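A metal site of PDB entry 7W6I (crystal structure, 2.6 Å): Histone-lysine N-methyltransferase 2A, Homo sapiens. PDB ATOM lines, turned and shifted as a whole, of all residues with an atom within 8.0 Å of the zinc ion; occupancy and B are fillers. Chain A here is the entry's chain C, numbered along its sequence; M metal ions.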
ATOM      1  N   ILE A  27     -15.267   7.569  14.914  1.00  0.00           N
ATOM      2  CA  ILE A  27     -14.616   6.279  14.742  1.00  0.00           C
ATOM      3  C   ILE A  27     -13.989   6.183  13.359  1.00  0.00           C
ATOM      4  O   ILE A  27     -12.767   6.025  13.225  1.00  0.00           O
ATOM      5  CB  ILE A  27     -15.620   5.137  14.972  1.00  0.00           C
ATOM      6  CG1 ILE A  27     -16.210   5.216  16.378  1.00  0.00           C
ATOM      7  CG2 ILE A  27     -14.949   3.796  14.750  1.00  0.00           C
ATOM      8  CD1 ILE A  27     -17.358   4.270  16.622  1.00  0.00           C
ATOM      9  N   HIS A  97     -17.462  -0.734  13.677  1.00  0.00           N
ATOM     10  CA  HIS A  97     -17.056  -1.764  14.612  1.00  0.00           C
ATOM     11  C   HIS A  97     -16.595  -1.143  15.931  1.00  0.00           C
ATOM     12  O   HIS A  97     -16.087  -0.016  15.960  1.00  0.00           O
ATOM     13  CB  HIS A  97     -15.938  -2.630  14.004  1.00  0.00           C
ATOM     14  CG  HIS A  97     -15.187  -3.448  15.009  1.00  0.00           C
ATOM     15  ND1 HIS A  97     -15.452  -4.778  15.224  1.00  0.00           N
ATOM     16  CD2 HIS A  97     -14.160  -3.119  15.837  1.00  0.00           C
ATOM     17  CE1 HIS A  97     -14.632  -5.236  16.159  1.00  0.00           C
ATOM     18  NE2 HIS A  97     -13.840  -4.254  16.544  1.00  0.00           N
ATOM     19  N   SER A  98     -16.780  -1.889  17.013  1.00  0.00           N
ATOM     20  CA  SER A  98     -16.248  -1.498  18.310  1.00  0.00           C
ATOM     21  C   SER A  98     -15.849  -2.748  19.077  1.00  0.00           C
ATOM     22  O   SER A  98     -16.345  -3.848  18.822  1.00  0.00           O
ATOM     23  CB  SER A  98     -17.245  -0.673  19.129  1.00  0.00           C
ATOM     24  OG  SER A  98     -16.844  -0.577  20.478  1.00  0.00           O
ATOM     25  N   CYS A  99     -14.940  -2.559  20.036  1.00  0.00           N
ATOM     26  CA  CYS A  99     -14.582  -3.604  20.985  1.00  0.00           C
ATOM     27  C   CYS A  99     -15.345  -3.476  22.303  1.00  0.00           C
ATOM     28  O   CYS A  99     -15.291  -4.414  23.123  1.00  0.00           O
ATOM     29  CB  CYS A  99     -13.076  -3.585  21.244  1.00  0.00           C
ATOM     30  SG  CYS A  99     -12.069  -3.364  19.737  1.00  0.00           S
ATOM     31  N   GLU A 100     -16.035  -2.365  22.516  1.00  0.00           N
ATOM     32  CA  GLU A 100     -17.060  -2.233  23.555  1.00  0.00           C
ATOM     33  C   GLU A 100     -18.393  -1.911  22.882  1.00  0.00           C
ATOM     34  O   GLU A 100     -18.953  -0.821  23.087  1.00  0.00           O
ATOM     35  CB  GLU A 100     -16.711  -1.141  24.568  1.00  0.00           C
ATOM     36  CG  GLU A 100     -15.343  -1.256  25.234  1.00  0.00           C
ATOM     37  CD  GLU A 100     -15.204  -2.440  26.167  1.00  0.00           C
ATOM     38  OE1 GLU A 100     -16.208  -3.136  26.418  1.00  0.00           O
ATOM     39  OE2 GLU A 100     -14.085  -2.669  26.659  1.00  0.00           O
ATOM     40  N   PRO A 146      -6.235  -1.492  11.343  1.00  0.00           N
ATOM     41  CA  PRO A 146      -6.269  -1.000  12.724  1.00  0.00           C
ATOM     42  C   PRO A 146      -7.658  -0.510  13.109  1.00  0.00           C
ATOM     43  O   PRO A 146      -8.407   0.010  12.284  1.00  0.00           O
ATOM     44  CB  PRO A 146      -5.239   0.141  12.724  1.00  0.00           C
ATOM     45  CG  PRO A 146      -4.369  -0.131  11.529  1.00  0.00           C
ATOM     46  CD  PRO A 146      -5.288  -0.728  10.512  1.00  0.00           C
ATOM     47  N   CYS A 147      -7.983  -0.674  14.390  1.00  0.00           N
ATOM     48  CA  CYS A 147      -9.297  -0.327  14.916  1.00  0.00           C
ATOM     49  C   CYS A 147      -9.216   0.995  15.673  1.00  0.00           C
ATOM     50  O   CYS A 147      -8.413   1.142  16.595  1.00  0.00           O
ATOM     51  CB  CYS A 147      -9.820  -1.426  15.829  1.00  0.00           C
ATOM     52  SG  CYS A 147     -11.401  -1.034  16.583  1.00  0.00           S
ATOM     53  N   ASN A 148     -10.058   1.945  15.278  1.00  0.00           N
ATOM     54  CA  ASN A 148     -10.133   3.273  15.878  1.00  0.00           C
ATOM     55  C   ASN A 148     -11.471   3.493  16.572  1.00  0.00           C
ATOM     56  O   ASN A 148     -12.079   4.562  16.470  1.00  0.00           O
ATOM     57  CB  ASN A 148      -9.887   4.355  14.823  1.00  0.00           C
ATOM     58  CG  ASN A 148      -9.566   5.704  15.443  1.00  0.00           C
ATOM     59  OD1 ASN A 148      -8.748   5.811  16.349  1.00  0.00           O
ATOM     60  ND2 ASN A 148     -10.234   6.746  14.947  1.00  0.00           N
ATOM     61  N   CYS A 149     -11.942   2.479  17.304  1.00  0.00           N
ATOM     62  CA  CYS A 149     -13.218   2.579  17.996  1.00  0.00           C
ATOM     63  C   CYS A 149     -13.130   3.436  19.260  1.00  0.00           C
ATOM     64  O   CYS A 149     -14.186   3.802  19.807  1.00  0.00           O
ATOM     65  CB  CYS A 149     -13.727   1.182  18.353  1.00  0.00           C
ATOM     66  SG  CYS A 149     -12.753   0.348  19.605  1.00  0.00           S
ATOM     67  N   GLY A 150     -11.932   3.747  19.739  1.00  0.00           N
ATOM     68  CA  GLY A 150     -11.782   4.553  20.924  1.00  0.00           C
ATOM     69  C   GLY A 150     -12.115   3.866  22.225  1.00  0.00           C
ATOM     70  O   GLY A 150     -12.177   4.541  23.259  1.00  0.00           O
ATOM     71  N   ALA A 151     -12.330   2.560  22.209  1.00  0.00           N
ATOM     72  CA  ALA A 151     -12.655   1.843  23.422  1.00  0.00           C
ATOM     73  C   ALA A 151     -11.428   1.712  24.313  1.00  0.00           C
ATOM     74  O   ALA A 151     -10.297   1.596  23.832  1.00  0.00           O
ATOM     75  CB  ALA A 151     -13.211   0.463  23.094  1.00  0.00           C
ATOM     76  N   LYS A 152     -11.662   1.753  25.628  1.00  0.00           N
ATOM     77  CA  LYS A 152     -10.560   1.546  26.568  1.00  0.00           C
ATOM     78  C   LYS A 152      -9.953   0.158  26.423  1.00  0.00           C
ATOM     79  O   LYS A 152      -8.789  -0.047  26.775  1.00  0.00           O
ATOM     80  CB  LYS A 152     -11.044   1.738  28.002  1.00  0.00           C
ATOM     81  CG  LYS A 152     -11.882   2.982  28.217  1.00  0.00           C
ATOM     82  CD  LYS A 152     -12.216   3.153  29.690  1.00  0.00           C
ATOM     83  CE  LYS A 152     -11.132   3.944  30.409  1.00  0.00           C
ATOM     84  NZ  LYS A 152     -11.072   3.606  31.852  1.00  0.00           N
ATOM     85  N   LYS A 153     -10.705  -0.787  25.894  1.00  0.00           N
ATOM     86  CA  LYS A 153     -10.220  -2.160  25.753  1.00  0.00           C
ATOM     87  C   LYS A 153     -10.188  -2.600  24.295  1.00  0.00           C
ATOM     88  O   LYS A 153     -10.531  -3.734  23.949  1.00  0.00           O
ATOM     89  CB  LYS A 153     -11.067  -3.086  26.625  1.00  0.00           C
ATOM     90  CG  LYS A 153     -10.849  -2.744  28.058  1.00  0.00           C
ATOM     91  CD  LYS A 153     -11.656  -3.612  28.975  1.00  0.00           C
ATOM     92  CE  LYS A 153     -11.385  -3.145  30.380  1.00  0.00           C
ATOM     93  NZ  LYS A 153     -12.075  -3.990  31.335  1.00  0.00           N
ATOM     94  N   CYS A 154      -9.731  -1.693  23.445  1.00  0.00           N
ATOM     95  CA  CYS A 154      -9.718  -1.942  22.019  1.00  0.00           C
ATOM     96  C   CYS A 154      -8.701  -3.022  21.671  1.00  0.00           C
ATOM     97  O   CYS A 154      -7.609  -3.098  22.253  1.00  0.00           O
ATOM     98  CB  CYS A 154      -9.406  -0.654  21.269  1.00  0.00           C
ATOM     99  SG  CYS A 154      -9.104  -0.855  19.512  1.00  0.00           S
ATOM    100  N   ARG A 155      -9.065  -3.861  20.702  1.00  0.00           N
ATOM    101  CA  ARG A 155      -8.173  -4.903  20.204  1.00  0.00           C
ATOM    102  C   ARG A 155      -7.102  -4.350  19.275  1.00  0.00           C
ATOM    103  O   ARG A 155      -6.231  -5.112  18.856  1.00  0.00           O
ATOM    104  CB  ARG A 155      -8.986  -5.976  19.489  1.00  0.00           C
ATOM    105  CG  ARG A 155     -10.084  -6.591  20.346  1.00  0.00           C
ATOM    106  CD  ARG A 155     -10.528  -7.955  19.825  1.00  0.00           C
ATOM    107  NE  ARG A 155     -11.060  -7.896  18.473  1.00  0.00           N
ATOM    108  CZ  ARG A 155     -12.359  -7.893  18.170  1.00  0.00           C
ATOM    109  NH1 ARG A 155     -12.759  -7.850  16.907  1.00  0.00           N
ATOM    110  NH2 ARG A 155     -13.256  -7.934  19.142  1.00  0.00           N
ATOM    111  N   LYS A 156      -7.185  -3.060  18.931  1.00  0.00           N
ATOM    112  CA  LYS A 156      -6.202  -2.329  18.123  1.00  0.00           C
ATOM    113  C   LYS A 156      -6.291  -2.695  16.653  1.00  0.00           C
ATOM    114  O   LYS A 156      -5.669  -2.033  15.807  1.00  0.00           O
ATOM    115  CB  LYS A 156      -4.773  -2.578  18.645  1.00  0.00           C
ATOM    116  N   PHE A 157      -7.080  -3.709  16.308  1.00  0.00           N
ATOM    117  CA  PHE A 157      -7.287  -4.089  14.913  1.00  0.00           C
ATOM    118  C   PHE A 157      -8.685  -4.656  14.737  1.00  0.00           C
ATOM    119  O   PHE A 157      -9.259  -5.235  15.664  1.00  0.00           O
ATOM    120  CB  PHE A 157      -6.259  -5.119  14.423  1.00  0.00           C
ATOM    121  CG  PHE A 157      -4.825  -4.681  14.582  1.00  0.00           C
ATOM    122  CD1 PHE A 157      -4.262  -3.769  13.713  1.00  0.00           C
ATOM    123  CD2 PHE A 157      -4.044  -5.184  15.615  1.00  0.00           C
ATOM    124  CE1 PHE A 157      -2.950  -3.366  13.849  1.00  0.00           C
ATOM    125  CE2 PHE A 157      -2.729  -4.789  15.772  1.00  0.00           C
ATOM    126  CZ  PHE A 157      -2.178  -3.880  14.884  1.00  0.00           C
ATOM    127  N   LEU A 158      -9.229  -4.473  13.536  1.00  0.00           N
ATOM    128  CA  LEU A 158     -10.512  -5.084  13.199  1.00  0.00           C
ATOM    129  C   LEU A 158     -10.370  -6.599  13.045  1.00  0.00           C
ATOM    130  O   LEU A 158     -11.346  -7.334  13.245  1.00  0.00           O
ATOM    131  CB  LEU A 158     -11.074  -4.476  11.916  1.00  0.00           C
ATOM    132  CG  LEU A 158     -11.434  -2.986  11.922  1.00  0.00           C
ATOM    133  CD1 LEU A 158     -12.134  -2.599  10.620  1.00  0.00           C
ATOM    134  CD2 LEU A 158     -12.292  -2.652  13.119  1.00  0.00           C
HETATM  135 ZN    ZN M   1     -11.300  -1.319  18.885  1.00  0.00          ZN
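N of Arg 155 touches the zinc ion, at 3.8 Å. Of the 18 residues printed, 5 come within 4 Å of the zinc ion. The nearest printed residue that does not touch the zinc ion is Lys 156 (4.5 Å).
The zinc ion is bound by the side-chain sulfur of Cys 147, the side-chain sulfur of Cys 149, the side-chain sulfur of Cys 154 and the side-chain sulfur of Cys 99. The zinc ion has four donor atoms within binding distance.
The backbone NH (N) of Lys 156 sits close to the side-chain sulfur (SG) of Cys 154, at 3.0 Å. The side-chain sulfur (SG) of Cys 149 sits close to the backbone NH (N) of Ala 151. The side-chain sulfur (SG) of Cys 99 lies close to a ring nitrogen (NE2) of His 97. The backbone NH of Arg 155 sits close to the side-chain sulfur of Cys 99, 3.2 Å away. The backbone NH (N) of Cys 147 sits at hydrogen-bond distance from the backbone carbonyl oxygen (O) of Lys 156 (3.0 Å).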
